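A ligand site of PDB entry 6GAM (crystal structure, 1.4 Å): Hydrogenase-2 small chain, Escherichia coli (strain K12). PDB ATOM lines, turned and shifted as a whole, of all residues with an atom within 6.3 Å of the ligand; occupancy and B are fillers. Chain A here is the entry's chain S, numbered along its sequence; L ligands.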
ATOM      1  N   ILE A 191     -17.209  11.399  -5.992  1.00  0.00           N
ATOM      2  CA  ILE A 191     -17.500  10.434  -4.938  1.00  0.00           C
ATOM      3  C   ILE A 191     -18.035   9.109  -5.523  1.00  0.00           C
ATOM      4  O   ILE A 191     -17.577   8.031  -5.151  1.00  0.00           O
ATOM      5  CB  ILE A 191     -18.427  11.063  -3.865  1.00  0.00           C
ATOM      6  CG1 ILE A 191     -17.667  12.137  -3.106  1.00  0.00           C
ATOM      7  CG2 ILE A 191     -19.013  10.005  -2.960  1.00  0.00           C
ATOM      8  CD1 ILE A 191     -18.566  12.994  -2.224  1.00  0.00           C
ATOM      9  N   HIS A 192     -18.918   9.205  -6.525  1.00  0.00           N
ATOM     10  CA  HIS A 192     -19.474   7.998  -7.173  1.00  0.00           C
ATOM     11  C   HIS A 192     -18.468   7.205  -7.958  1.00  0.00           C
ATOM     12  O   HIS A 192     -18.714   6.044  -8.201  1.00  0.00           O
ATOM     13  CB  HIS A 192     -20.595   8.462  -8.081  1.00  0.00           C
ATOM     14  CG  HIS A 192     -21.359   7.405  -8.786  1.00  0.00           C
ATOM     15  ND1 HIS A 192     -22.353   6.635  -8.219  1.00  0.00           N
ATOM     16  CD2 HIS A 192     -21.342   7.109 -10.112  1.00  0.00           C
ATOM     17  CE1 HIS A 192     -22.891   5.871  -9.172  1.00  0.00           C
ATOM     18  NE2 HIS A 192     -22.282   6.140 -10.322  1.00  0.00           N
ATOM     19  N   GLU A 193     -17.344   7.821  -8.341  1.00  0.00           N
ATOM     20  CA  GLU A 193     -16.281   7.102  -9.019  1.00  0.00           C
ATOM     21  C   GLU A 193     -15.274   6.501  -8.038  1.00  0.00           C
ATOM     22  O   GLU A 193     -14.245   5.943  -8.444  1.00  0.00           O
ATOM     23  CB  GLU A 193     -15.616   7.977 -10.070  1.00  0.00           C
ATOM     24  CG  GLU A 193     -16.576   8.304 -11.224  1.00  0.00           C
ATOM     25  CD  GLU A 193     -17.100   7.074 -11.950  1.00  0.00           C
ATOM     26  OE1 GLU A 193     -18.341   6.908 -12.067  1.00  0.00           O
ATOM     27  OE2 GLU A 193     -16.265   6.255 -12.317  1.00  0.00           O
ATOM     28  N   CYS A 195     -16.908   4.991  -4.779  1.00  0.00           N
ATOM     29  CA  CYS A 195     -17.870   4.695  -3.704  1.00  0.00           C
ATOM     30  C   CYS A 195     -18.045   3.204  -3.554  1.00  0.00           C
ATOM     31  O   CYS A 195     -18.315   2.503  -4.554  1.00  0.00           O
ATOM     32  CB  CYS A 195     -19.245   5.315  -4.035  1.00  0.00           C
ATOM     33  SG  CYS A 195     -20.471   4.955  -2.748  1.00  0.00           S
ATOM     34  N   GLU A 196     -17.958   2.713  -2.322  1.00  0.00           N
ATOM     35  CA  GLU A 196     -18.132   1.300  -2.028  1.00  0.00           C
ATOM     36  C   GLU A 196     -19.503   0.733  -2.327  1.00  0.00           C
ATOM     37  O   GLU A 196     -19.666  -0.496  -2.343  1.00  0.00           O
ATOM     38  CB  GLU A 196     -17.678   0.990  -0.615  1.00  0.00           C
ATOM     39  CG  GLU A 196     -18.558   1.548   0.523  1.00  0.00           C
ATOM     40  CD  GLU A 196     -18.318   3.000   0.961  1.00  0.00           C
ATOM     41  OE1 GLU A 196     -17.600   3.774   0.234  1.00  0.00           O
ATOM     42  OE2 GLU A 196     -18.882   3.287   2.078  1.00  0.00           O
ATOM     43  N   ARG A 197     -20.505   1.599  -2.568  1.00  0.00           N
ATOM     44  CA  ARG A 197     -21.836   1.097  -2.894  1.00  0.00           C
ATOM     45  C   ARG A 197     -22.031   1.036  -4.388  1.00  0.00           C
ATOM     46  O   ARG A 197     -23.113   0.605  -4.809  1.00  0.00           O
ATOM     47  CB  ARG A 197     -22.938   1.907  -2.200  1.00  0.00           C
ATOM     48  CG  ARG A 197     -22.736   1.836  -0.680  1.00  0.00           C
ATOM     49  CD  ARG A 197     -23.904   2.355   0.076  1.00  0.00           C
ATOM     50  NE  ARG A 197     -23.653   2.192   1.507  1.00  0.00           N
ATOM     51  CZ  ARG A 197     -24.582   2.167   2.440  1.00  0.00           C
ATOM     52  NH1 ARG A 197     -25.858   2.385   2.163  1.00  0.00           N
ATOM     53  NH2 ARG A 197     -24.200   2.004   3.676  1.00  0.00           N
ATOM     54  N   ARG A 198     -20.999   1.342  -5.163  1.00  0.00           N
ATOM     55  CA  ARG A 198     -21.122   1.234  -6.617  1.00  0.00           C
ATOM     56  C   ARG A 198     -21.609  -0.145  -7.072  1.00  0.00           C
ATOM     57  O   ARG A 198     -22.407  -0.188  -8.050  1.00  0.00           O
ATOM     58  CB  ARG A 198     -19.845   1.637  -7.310  1.00  0.00           C
ATOM     59  CG  ARG A 198     -19.927   1.600  -8.849  1.00  0.00           C
ATOM     60  CD  ARG A 198     -20.946   2.564  -9.441  1.00  0.00           C
ATOM     61  NE  ARG A 198     -20.786   2.535 -10.895  1.00  0.00           N
ATOM     62  CZ  ARG A 198     -19.969   3.328 -11.560  1.00  0.00           C
ATOM     63  NH1 ARG A 198     -19.363   4.367 -11.001  1.00  0.00           N
ATOM     64  NH2 ARG A 198     -19.794   3.116 -12.861  1.00  0.00           N
ATOM     65  N   PRO A 199     -21.159  -1.246  -6.460  1.00  0.00           N
ATOM     66  CA  PRO A 199     -21.706  -2.548  -6.975  1.00  0.00           C
ATOM     67  C   PRO A 199     -23.230  -2.641  -6.901  1.00  0.00           C
ATOM     68  O   PRO A 199     -23.882  -3.291  -7.750  1.00  0.00           O
ATOM     69  CB  PRO A 199     -21.087  -3.564  -6.019  1.00  0.00           C
ATOM     70  CG  PRO A 199     -19.806  -2.885  -5.572  1.00  0.00           C
ATOM     71  CD  PRO A 199     -20.142  -1.438  -5.418  1.00  0.00           C
ATOM     72  N   PHE A 201     -25.364   0.016  -6.974  1.00  0.00           N
ATOM     73  CA  PHE A 201     -25.824   0.865  -8.093  1.00  0.00           C
ATOM     74  C   PHE A 201     -25.819   0.051  -9.384  1.00  0.00           C
ATOM     75  O   PHE A 201     -26.845   0.003 -10.119  1.00  0.00           O
ATOM     76  CB  PHE A 201     -24.919   2.076  -8.201  1.00  0.00           C
ATOM     77  CG  PHE A 201     -25.270   2.999  -9.326  1.00  0.00           C
ATOM     78  CD1 PHE A 201     -24.759   2.809 -10.587  1.00  0.00           C
ATOM     79  CD2 PHE A 201     -26.068   4.112  -9.096  1.00  0.00           C
ATOM     80  CE1 PHE A 201     -25.070   3.677 -11.623  1.00  0.00           C
ATOM     81  CE2 PHE A 201     -26.352   5.015 -10.139  1.00  0.00           C
ATOM     82  CZ  PHE A 201     -25.853   4.798 -11.402  1.00  0.00           C
ATOM     83  N   PHE A 206     -31.157  -0.821  -4.748  1.00  0.00           N
ATOM     84  CA  PHE A 206     -31.351   0.533  -4.258  1.00  0.00           C
ATOM     85  C   PHE A 206     -32.206   0.563  -3.023  1.00  0.00           C
ATOM     86  O   PHE A 206     -33.266  -0.065  -2.947  1.00  0.00           O
ATOM     87  CB  PHE A 206     -32.046   1.387  -5.300  1.00  0.00           C
ATOM     88  CG  PHE A 206     -31.281   1.593  -6.548  1.00  0.00           C
ATOM     89  CD1 PHE A 206     -30.112   2.310  -6.544  1.00  0.00           C
ATOM     90  CD2 PHE A 206     -31.745   1.098  -7.798  1.00  0.00           C
ATOM     91  CE1 PHE A 206     -29.391   2.563  -7.666  1.00  0.00           C
ATOM     92  CE2 PHE A 206     -31.028   1.349  -8.929  1.00  0.00           C
ATOM     93  CZ  PHE A 206     -29.845   2.061  -8.908  1.00  0.00           C
ATOM     94  N   TRP A 219     -27.460  -0.927   0.747  1.00  0.00           N
ATOM     95  CA  TRP A 219     -27.531  -0.758  -0.671  1.00  0.00           C
ATOM     96  C   TRP A 219     -27.319   0.684  -1.098  1.00  0.00           C
ATOM     97  O   TRP A 219     -27.241   1.619  -0.275  1.00  0.00           O
ATOM     98  CB  TRP A 219     -28.890  -1.270  -1.172  1.00  0.00           C
ATOM     99  CG  TRP A 219     -28.995  -2.790  -1.219  1.00  0.00           C
ATOM    100  CD1 TRP A 219     -28.066  -3.705  -0.792  1.00  0.00           C
ATOM    101  CD2 TRP A 219     -30.128  -3.553  -1.680  1.00  0.00           C
ATOM    102  NE1 TRP A 219     -28.577  -4.998  -0.958  1.00  0.00           N
ATOM    103  CE2 TRP A 219     -29.827  -4.900  -1.508  1.00  0.00           C
ATOM    104  CE3 TRP A 219     -31.347  -3.196  -2.248  1.00  0.00           C
ATOM    105  CZ2 TRP A 219     -30.737  -5.919  -1.893  1.00  0.00           C
ATOM    106  CZ3 TRP A 219     -32.232  -4.214  -2.634  1.00  0.00           C
ATOM    107  CH2 TRP A 219     -31.919  -5.534  -2.438  1.00  0.00           C
ATOM    108  N   CYS A 220     -27.226   0.899  -2.398  1.00  0.00           N
ATOM    109  CA  CYS A 220     -26.957   2.231  -2.915  1.00  0.00           C
ATOM    110  C   CYS A 220     -28.086   3.183  -2.618  1.00  0.00           C
ATOM    111  O   CYS A 220     -29.249   2.798  -2.594  1.00  0.00           O
ATOM    112  CB  CYS A 220     -26.666   2.169  -4.436  1.00  0.00           C
ATOM    113  SG  CYS A 220     -26.674   3.703  -5.364  1.00  0.00           S
ATOM    114  N   LEU A 221     -27.723   4.456  -2.401  1.00  0.00           N
ATOM    115  CA  LEU A 221     -28.619   5.519  -1.985  1.00  0.00           C
ATOM    116  C   LEU A 221     -29.008   6.469  -3.129  1.00  0.00           C
ATOM    117  O   LEU A 221     -29.601   7.534  -2.889  1.00  0.00           O
ATOM    118  CB  LEU A 221     -27.995   6.283  -0.804  1.00  0.00           C
ATOM    119  CG  LEU A 221     -27.559   5.386   0.365  1.00  0.00           C
ATOM    120  CD1 LEU A 221     -27.085   6.293   1.518  1.00  0.00           C
ATOM    121  CD2 LEU A 221     -28.605   4.445   0.836  1.00  0.00           C
ATOM    122  N   TYR A 222     -28.718   6.086  -4.382  1.00  0.00           N
ATOM    123  CA  TYR A 222     -29.035   6.949  -5.525  1.00  0.00           C
ATOM    124  C   TYR A 222     -30.493   7.380  -5.523  1.00  0.00           C
ATOM    125  O   TYR A 222     -30.791   8.566  -5.751  1.00  0.00           O
ATOM    126  CB  TYR A 222     -28.702   6.214  -6.848  1.00  0.00           C
ATOM    127  CG  TYR A 222     -29.036   7.061  -8.037  1.00  0.00           C
ATOM    128  CD1 TYR A 222     -28.268   8.137  -8.363  1.00  0.00           C
ATOM    129  CD2 TYR A 222     -30.196   6.815  -8.748  1.00  0.00           C
ATOM    130  CE1 TYR A 222     -28.575   8.965  -9.428  1.00  0.00           C
ATOM    131  CE2 TYR A 222     -30.544   7.644  -9.795  1.00  0.00           C
ATOM    132  CZ  TYR A 222     -29.727   8.731 -10.111  1.00  0.00           C
ATOM    133  OH  TYR A 222     -30.087   9.600 -11.168  1.00  0.00           O
ATOM    134  N   HIS A 223     -31.405   6.435  -5.315  1.00  0.00           N
ATOM    135  CA  HIS A 223     -32.834   6.772  -5.347  1.00  0.00           C
ATOM    136  C   HIS A 223     -33.364   7.477  -4.116  1.00  0.00           C
ATOM    137  O   HIS A 223     -34.520   7.884  -4.108  1.00  0.00           O
ATOM    138  CB  HIS A 223     -33.674   5.553  -5.725  1.00  0.00           C
ATOM    139  CG  HIS A 223     -33.656   5.302  -7.192  1.00  0.00           C
ATOM    140  ND1 HIS A 223     -34.375   6.087  -8.068  1.00  0.00           N
ATOM    141  CD2 HIS A 223     -32.971   4.412  -7.946  1.00  0.00           C
ATOM    142  CE1 HIS A 223     -34.105   5.715  -9.302  1.00  0.00           C
ATOM    143  NE2 HIS A 223     -33.259   4.692  -9.266  1.00  0.00           N
ATOM    144  N   CYS A 226     -28.860  10.601  -3.607  1.00  0.00           N
ATOM    145  CA  CYS A 226     -27.397  10.714  -3.454  1.00  0.00           C
ATOM    146  C   CYS A 226     -26.799  11.573  -4.572  1.00  0.00           C
ATOM    147  O   CYS A 226     -26.980  11.319  -5.788  1.00  0.00           O
ATOM    148  CB  CYS A 226     -26.768   9.354  -3.402  1.00  0.00           C
ATOM    149  SG  CYS A 226     -25.006   9.443  -2.997  1.00  0.00           S
ATOM    150  N   LYS A 227     -26.015  12.564  -4.168  1.00  0.00           N
ATOM    151  CA  LYS A 227     -25.344  13.454  -5.101  1.00  0.00           C
ATOM    152  C   LYS A 227     -23.925  13.061  -5.391  1.00  0.00           C
ATOM    153  O   LYS A 227     -23.168  13.772  -6.083  1.00  0.00           O
ATOM    154  CB  LYS A 227     -25.400  14.883  -4.586  1.00  0.00           C
ATOM    155  CG  LYS A 227     -26.819  15.392  -4.346  1.00  0.00           C
ATOM    156  CD  LYS A 227     -27.761  15.188  -5.534  1.00  0.00           C
ATOM    157  CE  LYS A 227     -29.067  15.909  -5.344  1.00  0.00           C
ATOM    158  NZ  LYS A 227     -29.762  15.546  -4.073  1.00  0.00           N
ATOM    159  N   GLY A 228     -23.537  11.878  -4.949  1.00  0.00           N
ATOM    160  CA  GLY A 228     -22.225  11.335  -5.257  1.00  0.00           C
ATOM    161  C   GLY A 228     -21.838  11.393  -6.740  1.00  0.00           C
ATOM    162  O   GLY A 228     -20.695  11.694  -7.088  1.00  0.00           O
ATOM    163  N   PRO A 229     -22.806  11.153  -7.643  1.00  0.00           N
ATOM    164  CA  PRO A 229     -22.467  11.207  -9.081  1.00  0.00           C
ATOM    165  C   PRO A 229     -22.064  12.561  -9.631  1.00  0.00           C
ATOM    166  O   PRO A 229     -21.511  12.645 -10.739  1.00  0.00           O
ATOM    167  CB  PRO A 229     -23.740  10.714  -9.727  1.00  0.00           C
ATOM    168  CG  PRO A 229     -24.367   9.805  -8.711  1.00  0.00           C
ATOM    169  CD  PRO A 229     -24.108  10.510  -7.406  1.00  0.00           C
ATOM    170  N   TRP A 247     -18.879   8.180   7.012  1.00  0.00           N
ATOM    171  CA  TRP A 247     -19.253   9.250   6.122  1.00  0.00           C
ATOM    172  C   TRP A 247     -20.758   9.178   5.906  1.00  0.00           C
ATOM    173  O   TRP A 247     -21.383   8.173   6.332  1.00  0.00           O
ATOM    174  CB  TRP A 247     -18.456   9.232   4.813  1.00  0.00           C
ATOM    175  CG  TRP A 247     -18.709   8.093   3.845  1.00  0.00           C
ATOM    176  CD1 TRP A 247     -18.410   6.760   3.982  1.00  0.00           C
ATOM    177  CD2 TRP A 247     -19.220   8.248   2.503  1.00  0.00           C
ATOM    178  NE1 TRP A 247     -18.664   6.093   2.792  1.00  0.00           N
ATOM    179  CE2 TRP A 247     -19.185   6.983   1.898  1.00  0.00           C
ATOM    180  CE3 TRP A 247     -19.672   9.324   1.773  1.00  0.00           C
ATOM    181  CZ2 TRP A 247     -19.596   6.810   0.544  1.00  0.00           C
ATOM    182  CZ3 TRP A 247     -20.073   9.140   0.472  1.00  0.00           C
ATOM    183  CH2 TRP A 247     -19.994   7.885  -0.134  1.00  0.00           C
ATOM    184  N   VAL A 249     -22.966   8.483   3.534  1.00  0.00           N
ATOM    185  CA  VAL A 249     -23.515   7.293   2.847  1.00  0.00           C
ATOM    186  C   VAL A 249     -23.314   6.056   3.697  1.00  0.00           C
ATOM    187  O   VAL A 249     -24.233   5.221   3.859  1.00  0.00           O
ATOM    188  CB  VAL A 249     -22.889   7.157   1.457  1.00  0.00           C
ATOM    189  CG1 VAL A 249     -23.124   5.749   0.909  1.00  0.00           C
ATOM    190  CG2 VAL A 249     -23.427   8.241   0.531  1.00  0.00           C
ATOM    191  N   PRO A 254     -27.961   9.760   1.929  1.00  0.00           N
ATOM    192  CA  PRO A 254     -27.307  10.190   0.691  1.00  0.00           C
ATOM    193  C   PRO A 254     -26.372  11.350   0.843  1.00  0.00           C
ATOM    194  O   PRO A 254     -26.553  12.204   1.710  1.00  0.00           O
ATOM    195  CB  PRO A 254     -28.508  10.562  -0.222  1.00  0.00           C
ATOM    196  CG  PRO A 254     -29.631  10.821   0.716  1.00  0.00           C
ATOM    197  CD  PRO A 254     -29.434   9.796   1.805  1.00  0.00           C
ATOM    198  N   CYS A 255     -25.340  11.417   0.002  1.00  0.00           N
ATOM    199  CA  CYS A 255     -24.589  12.652  -0.205  1.00  0.00           C
ATOM    200  C   CYS A 255     -25.539  13.740  -0.691  1.00  0.00           C
ATOM    201  O   CYS A 255     -26.448  13.454  -1.504  1.00  0.00           O
ATOM    202  CB  CYS A 255     -23.456  12.447  -1.211  1.00  0.00           C
ATOM    203  SG  CYS A 255     -22.540  13.938  -1.699  1.00  0.00           S
HETATM  204 FE1  LIG L   1     -24.816   4.952  -4.901  1.00  0.00          FE
HETATM  205 FE2  LIG L   1     -24.223   7.512  -4.028  1.00  0.00          FE
HETATM  206 FE3  LIG L   1     -23.033   6.514  -6.276  1.00  0.00          FE
HETATM  207 FE4  LIG L   1     -22.350   5.555  -3.865  1.00  0.00          FE
HETATM  208  S1  LIG L   1     -22.029   7.710  -4.656  1.00  0.00           S
HETATM  209  S2  LIG L   1     -22.788   4.266  -5.704  1.00  0.00           S
HETATM  210  S3  LIG L   1     -24.384   5.572  -2.763  1.00  0.00           S
HETATM  211  S4  LIG L   1     -25.234   7.003  -5.976  1.00  0.00           S
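A ring nitrogen (ND1) of His 192 binds an iron atom (FE3) of the ligand (2.1 Å). An iron atom (FE4) of the ligand is bound by the side-chain sulfur (SG) of Cys 195, 2.3 Å away. SG of Cys 220 binds FE1 of the ligand, 2.3 Å away. FE2 of the ligand is bound by SG of Cys 226 (2.3 Å). A sulfur (S2) of the ligand lies close to the backbone NH (N) of Arg 198 (3.5 Å). The backbone NH (N) of Leu 221 sits close to a sulfur (S3) of the ligand (3.5 Å).
SG of Cys 195 lies close to N of Arg 197, 3.4 Å away. The side-chain sulfur (SG) of Cys 220 sits close to the backbone NH (N) of Tyr 222. N of Cys 226 sits at hydrogen-bond distance from O of Leu 221, at 3.2 Å. The side-chain sulfur (SG) of Cys 226 sits close to the backbone NH (N) of Gly 228, 3.4 Å away. SG of Cys 226 lies close to N of Cys 255. The guanidinium group (NH1) of Arg 198 lies within salt-bridge range of the side-chain carboxylate (OE1) of Glu 193 (2.9 Å). The backbone carbonyl oxygen (O) of Val 249 is in hydrogen-bond range of the guanidinium group (NH2) of Arg 197, at 3.2 Å. The backbone carbonyl oxygen of Trp 219 lies within hydrogen-bond range of the guanidinium group of Arg 197 (2.9 Å).
The backbone carbonyl oxygen (O) of Arg 197 sits close to a sulfur (S2) of the ligand, 3.8 Å away. Phe 201 touches the ligand (CB to S2, 3.9 Å). Tyr 222 touches the ligand. Gly 228 touches the ligand. CD of Pro 229 touches S4 of the ligand, 3.95 Å away. Val 249 touches the ligand (CG1 to S3, 3.9 Å). Hydrophobic or aromatic side chains that line the ligand: His 192, Phe 201, Tyr 222, Pro 229 and Val 249. Within 4 Å of the ligand: His 192, Cys 195, Arg 197, Arg 198, Phe 201, Cys 220, Leu 221, Tyr 222, Cys 226, Gly 228, Pro 229 and Val 249.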
